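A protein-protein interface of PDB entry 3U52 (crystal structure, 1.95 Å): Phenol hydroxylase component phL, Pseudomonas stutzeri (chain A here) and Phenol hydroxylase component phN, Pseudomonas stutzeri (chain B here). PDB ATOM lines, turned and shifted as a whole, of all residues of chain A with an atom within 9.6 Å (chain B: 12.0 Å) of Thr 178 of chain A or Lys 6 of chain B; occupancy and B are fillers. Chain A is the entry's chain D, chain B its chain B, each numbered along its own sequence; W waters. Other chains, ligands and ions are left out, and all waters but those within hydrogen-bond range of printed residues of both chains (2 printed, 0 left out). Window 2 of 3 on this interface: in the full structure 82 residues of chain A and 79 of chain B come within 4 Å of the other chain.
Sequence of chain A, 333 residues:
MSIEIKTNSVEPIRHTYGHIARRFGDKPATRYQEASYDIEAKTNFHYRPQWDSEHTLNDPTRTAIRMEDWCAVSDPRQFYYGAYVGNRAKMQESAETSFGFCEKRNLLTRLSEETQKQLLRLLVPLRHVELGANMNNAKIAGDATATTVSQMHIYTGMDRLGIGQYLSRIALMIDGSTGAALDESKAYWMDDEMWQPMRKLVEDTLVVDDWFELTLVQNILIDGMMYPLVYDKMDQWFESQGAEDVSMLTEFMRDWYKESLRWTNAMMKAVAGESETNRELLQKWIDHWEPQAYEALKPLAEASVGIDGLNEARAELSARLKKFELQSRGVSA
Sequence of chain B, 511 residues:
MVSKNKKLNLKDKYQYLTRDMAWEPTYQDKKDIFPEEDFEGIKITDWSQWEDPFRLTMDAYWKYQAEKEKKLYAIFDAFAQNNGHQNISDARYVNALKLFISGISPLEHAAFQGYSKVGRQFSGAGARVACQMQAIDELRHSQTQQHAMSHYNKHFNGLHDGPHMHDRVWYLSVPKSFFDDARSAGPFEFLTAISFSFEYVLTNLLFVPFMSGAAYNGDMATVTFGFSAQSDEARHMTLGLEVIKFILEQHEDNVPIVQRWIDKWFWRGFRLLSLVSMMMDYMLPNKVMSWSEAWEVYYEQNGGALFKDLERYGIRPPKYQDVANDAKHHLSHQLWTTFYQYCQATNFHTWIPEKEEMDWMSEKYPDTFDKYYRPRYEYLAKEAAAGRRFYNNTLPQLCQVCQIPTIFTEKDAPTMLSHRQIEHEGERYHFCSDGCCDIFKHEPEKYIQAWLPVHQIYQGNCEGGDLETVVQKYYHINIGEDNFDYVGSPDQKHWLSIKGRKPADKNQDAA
The side-chain hydroxyl (OG1) of Thr 178 of chain A sits at hydrogen-bond distance from the backbone carbonyl oxygen (O) of Lys 6 of chain B, 3.2 Å away. N of Leu 8 of chain B is in hydrogen-bond range of O of Ser 177 of chain A (2.8 Å). The side-chain hydroxyl of Ser 177 of chain A lies within hydrogen-bond range of the side-chain amino group of Lys 13 of chain B. The side-chain carboxylate (OD1) of Asp 183 of chain A is in hydrogen-bond range of the side-chain hydroxyl (OH) of Tyr 16 of chain B, 2.8 Å away.
The backbone carbonyl oxygen (O) of Leu 172 of chain A is in hydrogen-bond range of the backbone NH (N) of Ser 177 of chain A, 2.7 Å away. OD1 of Asp 175 of chain A sits at hydrogen-bond distance from N of Ser 177 of chain A (2.9 Å). N of Thr 178 of chain A lies within hydrogen-bond range of OD1 of Asp 175 of chain A (2.8 Å). The side-chain carboxylate (OD2) of Asp 175 of chain A is in hydrogen-bond range of the backbone NH (N) of Gly 179 of chain A (3.0 Å).
Among the printed residues, pairs that only touch across the chains: Ser 168 of chain A with Leu 17 of chain B (3.5 Å), Leu 172 of chain A with Leu 8 of chain B (3.8 Å), Leu 172 of chain A with Leu 17 of chain B (3.97 Å), Gly 176 of chain A with Lys 7 of chain B (3.8 Å), Ser 177 of chain A with Lys 7 of chain B (3.6 Å), Thr 178 of chain A with Leu 8 of chain B (3.4 Å), Gly 179 of chain A with Leu 8 of chain B (3.7 Å), Gly 179 of chain A with Tyr 16 of chain B (3.8 Å) and Leu 182 of chain A with Tyr 16 of chain B (3.7 Å).
Printed residues of chain B within 4 Å of Ser 168 of chain A: Leu 17. Of chain B, only Leu 8 (3.8 Å) and Leu 17 (3.97 Å) come within 4 Å of Leu 172 of chain A. Ser 177 of chain A touches three residues of chain B. Gly 179 of chain A touches just these residues of chain B: Leu 8 and Tyr 16. Ala 180 of chain A touches none of the printed residues of chain B. Of the printed residues of chain B, Leu 182 of chain A touches Tyr 16. Of chain A, only Thr 178 comes within 4 Å of Lys 6 of chain B. Of the printed residues of chain A, Lys 7 of chain B touches Gly 176 (3.8 Å) and Ser 177 (3.6 Å). Asn 9 of chain B touches none of the printed residues of chain A. Lys 11 of chain B touches none of the printed residues of chain A. Of the printed residues of chain A, Lys 13 of chain B touches Ser 177. The nearest residue of chain B that does not touch Thr 178 of chain A is Lys 7 of chain B (4.2 Å). The nearest printed residue of chain A that does not touch Leu 8 of chain B is Asp 175 of chain A (5.8 Å).
Hydrophobic or aromatic side chains of chain B that line the printed part of chain A: Leu 8, Tyr 16 and Leu 17. Along chain B the printed residues that touch a printed residue of chain A span positions 6 to 17. Of the 18 printed residues of chain A, 8 touch a printed residue of chain B. Printed residues of chain A that touch a printed residue of chain B: Ser 168, Leu 172, Gly 176, Ser 177, Thr 178, Gly 179, Leu 182 and Asp 183. Among the printed residues, 13 pairs touch across the chains.
Water W1 bridges O of Leu 8 of chain B (2.6 Å) and OG of Ser 177 of chain A (2.7 Å). Water W2 bridges the backbone carbonyl oxygen of Thr 178 of chain A (2.7 Å) and the backbone carbonyl oxygen of Lys 6 of chain B (2.7 Å).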
ATOM      1  N   GLU A 103     -12.421  10.408  -4.777  1.00  0.00           N
ATOM      2  CA  GLU A 103     -12.957  10.976  -5.990  1.00  0.00           C
ATOM      3  C   GLU A 103     -12.774  12.511  -6.013  1.00  0.00           C
ATOM      4  O   GLU A 103     -12.240  13.028  -6.987  1.00  0.00           O
ATOM      5  CB  GLU A 103     -14.428  10.546  -6.183  1.00  0.00           C
ATOM      6  CG  GLU A 103     -15.265  11.340  -7.195  1.00  0.00           C
ATOM      7  CD  GLU A 103     -14.963  10.990  -8.638  1.00  0.00           C
ATOM      8  OE1 GLU A 103     -15.880  10.513  -9.353  1.00  0.00           O
ATOM      9  OE2 GLU A 103     -13.804  11.198  -9.068  1.00  0.00           O
ATOM     10  N   SER A 168     -15.332  -2.591  -8.696  1.00  0.00           N
ATOM     11  CA  SER A 168     -15.796  -1.881  -9.886  1.00  0.00           C
ATOM     12  C   SER A 168     -15.649  -0.355  -9.838  1.00  0.00           C
ATOM     13  O   SER A 168     -15.216   0.294 -10.813  1.00  0.00           O
ATOM     14  CB  SER A 168     -17.245  -2.220 -10.149  1.00  0.00           C
ATOM     15  OG  SER A 168     -17.366  -3.610 -10.330  1.00  0.00           O
ATOM     16  N   ARG A 169     -16.057   0.242  -8.717  1.00  0.00           N
ATOM     17  CA  ARG A 169     -16.021   1.684  -8.593  1.00  0.00           C
ATOM     18  C   ARG A 169     -14.621   2.262  -8.547  1.00  0.00           C
ATOM     19  O   ARG A 169     -14.394   3.394  -8.955  1.00  0.00           O
ATOM     20  CB  ARG A 169     -16.777   2.105  -7.341  1.00  0.00           C
ATOM     21  CG  ARG A 169     -18.283   2.079  -7.574  1.00  0.00           C
ATOM     22  CD  ARG A 169     -18.827   3.238  -6.817  1.00  0.00           C
ATOM     23  NE  ARG A 169     -19.534   2.734  -5.693  1.00  0.00           N
ATOM     24  CZ  ARG A 169     -19.773   3.384  -4.564  1.00  0.00           C
ATOM     25  NH1 ARG A 169     -19.289   4.605  -4.313  1.00  0.00           N
ATOM     26  NH2 ARG A 169     -20.490   2.741  -3.667  1.00  0.00           N
ATOM     27  N   ILE A 170     -13.685   1.501  -8.035  1.00  0.00           N
ATOM     28  CA  ILE A 170     -12.286   1.916  -8.104  1.00  0.00           C
ATOM     29  C   ILE A 170     -11.906   2.120  -9.572  1.00  0.00           C
ATOM     30  O   ILE A 170     -11.287   3.127  -9.938  1.00  0.00           O
ATOM     31  CB  ILE A 170     -11.384   0.841  -7.486  1.00  0.00           C
ATOM     32  CG1 ILE A 170     -11.600   0.799  -5.959  1.00  0.00           C
ATOM     33  CG2 ILE A 170      -9.935   1.084  -7.893  1.00  0.00           C
ATOM     34  CD1 ILE A 170     -10.723  -0.181  -5.249  1.00  0.00           C
ATOM     35  N   ALA A 171     -12.303   1.184 -10.433  1.00  0.00           N
ATOM     36  CA  ALA A 171     -11.988   1.310 -11.850  1.00  0.00           C
ATOM     37  C   ALA A 171     -12.696   2.496 -12.445  1.00  0.00           C
ATOM     38  O   ALA A 171     -12.099   3.230 -13.245  1.00  0.00           O
ATOM     39  CB  ALA A 171     -12.338   0.057 -12.582  1.00  0.00           C
ATOM     40  N   LEU A 172     -13.963   2.706 -12.055  1.00  0.00           N
ATOM     41  CA  LEU A 172     -14.730   3.846 -12.517  1.00  0.00           C
ATOM     42  C   LEU A 172     -14.123   5.160 -12.058  1.00  0.00           C
ATOM     43  O   LEU A 172     -14.224   6.176 -12.755  1.00  0.00           O
ATOM     44  CB  LEU A 172     -16.195   3.751 -12.068  1.00  0.00           C
ATOM     45  CG  LEU A 172     -16.971   2.709 -12.869  1.00  0.00           C
ATOM     46  CD1 LEU A 172     -18.414   2.553 -12.366  1.00  0.00           C
ATOM     47  CD2 LEU A 172     -16.963   3.026 -14.399  1.00  0.00           C
ATOM     48  N   MET A 173     -13.508   5.143 -10.885  1.00  0.00           N
ATOM     49  CA  MET A 173     -12.823   6.310 -10.401  1.00  0.00           C
ATOM     50  C   MET A 173     -11.649   6.582 -11.319  1.00  0.00           C
ATOM     51  O   MET A 173     -11.451   7.704 -11.722  1.00  0.00           O
ATOM     52  CB  MET A 173     -12.328   6.098  -8.965  1.00  0.00           C
ATOM     53  CG  MET A 173     -12.144   7.401  -8.268  1.00  0.00           C
ATOM     54  SD  MET A 173     -11.642   7.236  -6.568  1.00  0.00           S
ATOM     55  CE  MET A 173     -12.997   6.273  -5.892  1.00  0.00           C
ATOM     56  N   ILE A 174     -10.876   5.542 -11.654  1.00  0.00           N
ATOM     57  CA  ILE A 174      -9.700   5.677 -12.521  1.00  0.00           C
ATOM     58  C   ILE A 174     -10.022   6.163 -13.924  1.00  0.00           C
ATOM     59  O   ILE A 174      -9.231   6.938 -14.484  1.00  0.00           O
ATOM     60  CB  ILE A 174      -8.910   4.353 -12.606  1.00  0.00           C
ATOM     61  CG1 ILE A 174      -8.226   4.077 -11.273  1.00  0.00           C
ATOM     62  CG2 ILE A 174      -7.915   4.384 -13.783  1.00  0.00           C
ATOM     63  CD1 ILE A 174      -7.660   2.678 -11.116  1.00  0.00           C
ATOM     64  N   ASP A 175     -11.162   5.746 -14.499  1.00  0.00           N
ATOM     65  CA  ASP A 175     -11.555   6.218 -15.836  1.00  0.00           C
ATOM     66  C   ASP A 175     -12.509   7.412 -15.880  1.00  0.00           C
ATOM     67  O   ASP A 175     -12.967   7.802 -16.966  1.00  0.00           O
ATOM     68  CB  ASP A 175     -12.102   5.085 -16.721  1.00  0.00           C
ATOM     69  CG  ASP A 175     -13.470   4.540 -16.254  1.00  0.00           C
ATOM     70  OD1 ASP A 175     -14.335   5.306 -15.754  1.00  0.00           O
ATOM     71  OD2 ASP A 175     -13.696   3.322 -16.423  1.00  0.00           O
ATOM     72  N   GLY A 176     -12.840   7.957 -14.713  1.00  0.00           N
ATOM     73  CA  GLY A 176     -13.709   9.100 -14.660  1.00  0.00           C
ATOM     74  C   GLY A 176     -15.142   8.793 -15.033  1.00  0.00           C
ATOM     75  O   GLY A 176     -15.808   9.617 -15.661  1.00  0.00           O
ATOM     76  N   SER A 177     -15.612   7.606 -14.644  1.00  0.00           N
ATOM     77  CA  SER A 177     -17.027   7.211 -14.765  1.00  0.00           C
ATOM     78  C   SER A 177     -17.474   6.980 -16.231  1.00  0.00           C
ATOM     79  O   SER A 177     -18.617   7.246 -16.634  1.00  0.00           O
ATOM     80  CB  SER A 177     -17.924   8.184 -14.003  1.00  0.00           C
ATOM     81  OG  SER A 177     -19.218   7.643 -13.894  1.00  0.00           O
ATOM     82  N   THR A 178     -16.558   6.413 -16.991  1.00  0.00           N
ATOM     83  CA  THR A 178     -16.717   6.160 -18.404  1.00  0.00           C
ATOM     84  C   THR A 178     -16.879   4.631 -18.710  1.00  0.00           C
ATOM     85  O   THR A 178     -17.494   4.225 -19.706  1.00  0.00           O
ATOM     86  CB  THR A 178     -15.462   6.774 -19.063  1.00  0.00           C
ATOM     87  OG1 THR A 178     -15.815   7.722 -20.069  1.00  0.00           O
ATOM     88  CG2 THR A 178     -14.473   5.764 -19.523  1.00  0.00           C
ATOM     89  N   GLY A 179     -16.340   3.779 -17.838  1.00  0.00           N
ATOM     90  CA  GLY A 179     -16.394   2.328 -18.077  1.00  0.00           C
ATOM     91  C   GLY A 179     -15.179   1.756 -18.794  1.00  0.00           C
ATOM     92  O   GLY A 179     -14.983   0.544 -18.798  1.00  0.00           O
ATOM     93  N   ALA A 180     -14.348   2.634 -19.379  1.00  0.00           N
ATOM     94  CA  ALA A 180     -13.171   2.227 -20.145  1.00  0.00           C
ATOM     95  C   ALA A 180     -12.214   1.355 -19.334  1.00  0.00           C
ATOM     96  O   ALA A 180     -11.711   0.391 -19.861  1.00  0.00           O
ATOM     97  CB  ALA A 180     -12.420   3.468 -20.689  1.00  0.00           C
ATOM     98  N   ALA A 181     -11.996   1.686 -18.057  1.00  0.00           N
ATOM     99  CA  ALA A 181     -11.082   0.953 -17.185  1.00  0.00           C
ATOM    100  C   ALA A 181     -11.671  -0.397 -16.844  1.00  0.00           C
ATOM    101  O   ALA A 181     -10.938  -1.315 -16.554  1.00  0.00           O
ATOM    102  CB  ALA A 181     -10.760   1.732 -15.890  1.00  0.00           C
ATOM    103  N   LEU A 182     -12.997  -0.520 -16.880  1.00  0.00           N
ATOM    104  CA  LEU A 182     -13.636  -1.799 -16.600  1.00  0.00           C
ATOM    105  C   LEU A 182     -13.494  -2.743 -17.797  1.00  0.00           C
ATOM    106  O   LEU A 182     -13.276  -3.952 -17.639  1.00  0.00           O
ATOM    107  CB  LEU A 182     -15.095  -1.587 -16.288  1.00  0.00           C
ATOM    108  CG  LEU A 182     -15.616  -1.710 -14.858  1.00  0.00           C
ATOM    109  CD1 LEU A 182     -14.636  -2.059 -13.761  1.00  0.00           C
ATOM    110  CD2 LEU A 182     -16.510  -0.574 -14.506  1.00  0.00           C
ATOM    111  N   ASP A 183     -13.614  -2.176 -18.990  1.00  0.00           N
ATOM    112  CA  ASP A 183     -13.317  -2.908 -20.246  1.00  0.00           C
ATOM    113  C   ASP A 183     -11.893  -3.474 -20.234  1.00  0.00           C
ATOM    114  O   ASP A 183     -11.667  -4.641 -20.539  1.00  0.00           O
ATOM    115  CB  ASP A 183     -13.514  -1.986 -21.460  1.00  0.00           C
ATOM    116  CG  ASP A 183     -14.967  -1.570 -21.671  1.00  0.00           C
ATOM    117  OD1 ASP A 183     -15.893  -2.094 -20.991  1.00  0.00           O
ATOM    118  OD2 ASP A 183     -15.226  -0.725 -22.573  1.00  0.00           O
ATOM    119  N   GLU A 184     -10.932  -2.637 -19.865  1.00  0.00           N
ATOM    120  CA  GLU A 184      -9.531  -3.009 -19.868  1.00  0.00           C
ATOM    121  C   GLU A 184      -9.255  -4.147 -18.896  1.00  0.00           C
ATOM    122  O   GLU A 184      -8.560  -5.106 -19.238  1.00  0.00           O
ATOM    123  CB  GLU A 184      -8.681  -1.782 -19.537  1.00  0.00           C
ATOM    124  CG  GLU A 184      -7.218  -2.086 -19.290  1.00  0.00           C
ATOM    125  CD  GLU A 184      -6.357  -0.833 -19.118  1.00  0.00           C
ATOM    126  OE1 GLU A 184      -6.846   0.286 -19.410  1.00  0.00           O
ATOM    127  OE2 GLU A 184      -5.192  -0.978 -18.678  1.00  0.00           O
ATOM    128  N   LYS B   6     -17.691  11.477 -22.513  1.00  0.00           N
ATOM    129  CA  LYS B   6     -18.138  10.049 -22.609  1.00  0.00           C
ATOM    130  C   LYS B   6     -18.724   9.444 -21.294  1.00  0.00           C
ATOM    131  O   LYS B   6     -18.809   8.217 -21.177  1.00  0.00           O
ATOM    132  CB  LYS B   6     -16.965   9.182 -23.150  1.00  0.00           C
ATOM    133  N   LYS B   7     -19.123  10.283 -20.325  1.00  0.00           N
ATOM    134  CA  LYS B   7     -19.602   9.770 -19.026  1.00  0.00           C
ATOM    135  C   LYS B   7     -20.808   8.855 -19.139  1.00  0.00           C
ATOM    136  O   LYS B   7     -21.736   9.138 -19.890  1.00  0.00           O
ATOM    137  CB  LYS B   7     -19.925  10.873 -18.018  1.00  0.00           C
ATOM    138  CG  LYS B   7     -18.722  11.464 -17.337  1.00  0.00           C
ATOM    139  CD  LYS B   7     -19.157  12.428 -16.277  1.00  0.00           C
ATOM    140  CE  LYS B   7     -17.964  13.250 -15.801  1.00  0.00           C
ATOM    141  NZ  LYS B   7     -18.242  14.712 -15.961  1.00  0.00           N
ATOM    142  N   LEU B   8     -20.779   7.773 -18.366  1.00  0.00           N
ATOM    143  CA  LEU B   8     -21.880   6.812 -18.296  1.00  0.00           C
ATOM    144  C   LEU B   8     -23.166   7.425 -17.779  1.00  0.00           C
ATOM    145  O   LEU B   8     -23.163   8.087 -16.725  1.00  0.00           O
ATOM    146  CB  LEU B   8     -21.484   5.633 -17.390  1.00  0.00           C
ATOM    147  CG  LEU B   8     -20.377   4.688 -17.887  1.00  0.00           C
ATOM    148  CD1 LEU B   8     -19.876   3.812 -16.767  1.00  0.00           C
ATOM    149  CD2 LEU B   8     -20.850   3.845 -19.079  1.00  0.00           C
ATOM    150  N   ASN B   9     -24.282   7.189 -18.477  1.00  0.00           N
ATOM    151  CA  ASN B   9     -25.574   7.497 -17.876  1.00  0.00           C
ATOM    152  C   ASN B   9     -25.938   6.539 -16.725  1.00  0.00           C
ATOM    153  O   ASN B   9     -25.206   5.580 -16.492  1.00  0.00           O
ATOM    154  CB  ASN B   9     -26.679   7.778 -18.914  1.00  0.00           C
ATOM    155  CG  ASN B   9     -27.204   6.557 -19.622  1.00  0.00           C
ATOM    156  OD1 ASN B   9     -27.822   6.684 -20.682  1.00  0.00           O
ATOM    157  ND2 ASN B   9     -27.023   5.379 -19.033  1.00  0.00           N
ATOM    158  N   LEU B  10     -27.018   6.804 -15.992  1.00  0.00           N
ATOM    159  CA  LEU B  10     -27.349   5.983 -14.818  1.00  0.00           C
ATOM    160  C   LEU B  10     -27.648   4.528 -15.162  1.00  0.00           C
ATOM    161  O   LEU B  10     -27.245   3.638 -14.418  1.00  0.00           O
ATOM    162  CB  LEU B  10     -28.544   6.518 -14.059  1.00  0.00           C
ATOM    163  CG  LEU B  10     -28.501   7.792 -13.233  1.00  0.00           C
ATOM    164  CD1 LEU B  10     -29.695   7.687 -12.286  1.00  0.00           C
ATOM    165  CD2 LEU B  10     -27.191   8.056 -12.470  1.00  0.00           C
ATOM    166  N   LYS B  11     -28.391   4.302 -16.246  1.00  0.00           N
ATOM    167  CA  LYS B  11     -28.701   2.945 -16.691  1.00  0.00           C
ATOM    168  C   LYS B  11     -27.436   2.154 -16.994  1.00  0.00           C
ATOM    169  O   LYS B  11     -27.267   1.047 -16.476  1.00  0.00           O
ATOM    170  CB  LYS B  11     -29.616   2.952 -17.910  1.00  0.00           C
ATOM    171  CG  LYS B  11     -29.622   1.661 -18.695  1.00  0.00           C
ATOM    172  CD  LYS B  11     -30.653   1.682 -19.815  1.00  0.00           C
ATOM    173  CE  LYS B  11     -30.334   0.577 -20.821  1.00  0.00           C
ATOM    174  NZ  LYS B  11     -31.237   0.698 -21.999  1.00  0.00           N
ATOM    175  N   ASP B  12     -26.558   2.728 -17.818  1.00  0.00           N
ATOM    176  CA  ASP B  12     -25.294   2.130 -18.201  1.00  0.00           C
ATOM    177  C   ASP B  12     -24.313   1.961 -17.045  1.00  0.00           C
ATOM    178  O   ASP B  12     -23.622   0.939 -16.964  1.00  0.00           O
ATOM    179  CB  ASP B  12     -24.653   2.929 -19.347  1.00  0.00           C
ATOM    180  CG  ASP B  12     -25.418   2.772 -20.676  1.00  0.00           C
ATOM    181  OD1 ASP B  12     -25.243   3.621 -21.583  1.00  0.00           O
ATOM    182  OD2 ASP B  12     -26.199   1.795 -20.820  1.00  0.00           O
ATOM    183  N   LYS B  13     -24.227   2.942 -16.150  1.00  0.00           N
ATOM    184  CA  LYS B  13     -23.435   2.758 -14.923  1.00  0.00           C
ATOM    185  C   LYS B  13     -23.914   1.585 -14.066  1.00  0.00           C
ATOM    186  O   LYS B  13     -23.091   0.788 -13.615  1.00  0.00           O
ATOM    187  CB  LYS B  13     -23.342   4.055 -14.106  1.00  0.00           C
ATOM    188  CG  LYS B  13     -22.461   4.015 -12.848  1.00  0.00           C
ATOM    189  CD  LYS B  13     -21.935   5.447 -12.514  1.00  0.00           C
ATOM    190  CE  LYS B  13     -21.125   5.487 -11.179  1.00  0.00           C
ATOM    191  NZ  LYS B  13     -20.118   6.643 -11.080  1.00  0.00           N
ATOM    192  N   TYR B  14     -25.224   1.462 -13.841  1.00  0.00           N
ATOM    193  CA  TYR B  14     -25.759   0.366 -13.045  1.00  0.00           C
ATOM    194  C   TYR B  14     -25.382  -0.966 -13.692  1.00  0.00           C
ATOM    195  O   TYR B  14     -24.914  -1.887 -13.010  1.00  0.00           O
ATOM    196  CB  TYR B  14     -27.281   0.472 -12.861  1.00  0.00           C
ATOM    197  CG  TYR B  14     -27.810  -0.637 -11.972  1.00  0.00           C
ATOM    198  CD1 TYR B  14     -28.557  -1.686 -12.511  1.00  0.00           C
ATOM    199  CD2 TYR B  14     -27.533  -0.642 -10.600  1.00  0.00           C
ATOM    200  CE1 TYR B  14     -29.046  -2.707 -11.710  1.00  0.00           C
ATOM    201  CE2 TYR B  14     -27.997  -1.652  -9.779  1.00  0.00           C
ATOM    202  CZ  TYR B  14     -28.768  -2.685 -10.342  1.00  0.00           C
ATOM    203  OH  TYR B  14     -29.237  -3.729  -9.572  1.00  0.00           O
ATOM    204  N   GLN B  15     -25.515  -1.043 -15.013  1.00  0.00           N
ATOM    205  CA  GLN B  15     -25.119  -2.246 -15.767  1.00  0.00           C
ATOM    206  C   GLN B  15     -23.641  -2.610 -15.590  1.00  0.00           C
ATOM    207  O   GLN B  15     -23.335  -3.756 -15.336  1.00  0.00           O
ATOM    208  CB  GLN B  15     -25.540  -2.137 -17.240  1.00  0.00           C
ATOM    209  CG  GLN B  15     -27.044  -2.281 -17.414  1.00  0.00           C
ATOM    210  CD  GLN B  15     -27.511  -2.423 -18.875  1.00  0.00           C
ATOM    211  OE1 GLN B  15     -28.702  -2.230 -19.167  1.00  0.00           O
ATOM    212  NE2 GLN B  15     -26.599  -2.793 -19.780  1.00  0.00           N
ATOM    213  N   TYR B  16     -22.730  -1.634 -15.675  1.00  0.00           N
ATOM    214  CA  TYR B  16     -21.342  -1.854 -15.305  1.00  0.00           C
ATOM    215  C   TYR B  16     -21.120  -2.341 -13.886  1.00  0.00           C
ATOM    216  O   TYR B  16     -20.132  -3.030 -13.632  1.00  0.00           O
ATOM    217  CB  TYR B  16     -20.464  -0.627 -15.557  1.00  0.00           C
ATOM    218  CG  TYR B  16     -19.841  -0.637 -16.935  1.00  0.00           C
ATOM    219  CD1 TYR B  16     -20.327   0.195 -17.922  1.00  0.00           C
ATOM    220  CD2 TYR B  16     -18.770  -1.496 -17.258  1.00  0.00           C
ATOM    221  CE1 TYR B  16     -19.762   0.229 -19.185  1.00  0.00           C
ATOM    222  CE2 TYR B  16     -18.204  -1.471 -18.526  1.00  0.00           C
ATOM    223  CZ  TYR B  16     -18.714  -0.607 -19.473  1.00  0.00           C
ATOM    224  OH  TYR B  16     -18.224  -0.546 -20.739  1.00  0.00           O
ATOM    225  N   LEU B  17     -22.033  -2.036 -12.969  1.00  0.00           N
ATOM    226  CA  LEU B  17     -21.884  -2.495 -11.573  1.00  0.00           C
ATOM    227  C   LEU B  17     -22.616  -3.827 -11.271  1.00  0.00           C
ATOM    228  O   LEU B  17     -22.573  -4.352 -10.150  1.00  0.00           O
ATOM    229  CB  LEU B  17     -22.345  -1.382 -10.613  1.00  0.00           C
ATOM    230  CG  LEU B  17     -21.558  -0.067 -10.689  1.00  0.00           C
ATOM    231  CD1 LEU B  17     -22.235   1.096  -9.883  1.00  0.00           C
ATOM    232  CD2 LEU B  17     -20.149  -0.293 -10.204  1.00  0.00           C
ATOM    233  N   ASP B  20     -21.825  -6.432 -16.073  1.00  0.00           N
ATOM    234  CA  ASP B  20     -20.427  -6.476 -16.543  1.00  0.00           C
ATOM    235  C   ASP B  20     -19.428  -7.345 -15.701  1.00  0.00           C
ATOM    236  O   ASP B  20     -18.371  -7.715 -16.204  1.00  0.00           O
ATOM    237  CB  ASP B  20     -19.870  -5.063 -16.768  1.00  0.00           C
ATOM    238  CG  ASP B  20     -18.592  -5.087 -17.586  1.00  0.00           C
ATOM    239  OD1 ASP B  20     -17.503  -4.808 -17.034  1.00  0.00           O
ATOM    240  OD2 ASP B  20     -18.691  -5.481 -18.770  1.00  0.00           O
HETATM  241  O   HOH W   1     -21.630   8.609 -14.705  1.00  0.00           O
HETATM  242  O   HOH W   2     -18.516   5.602 -21.789  1.00  0.00           O
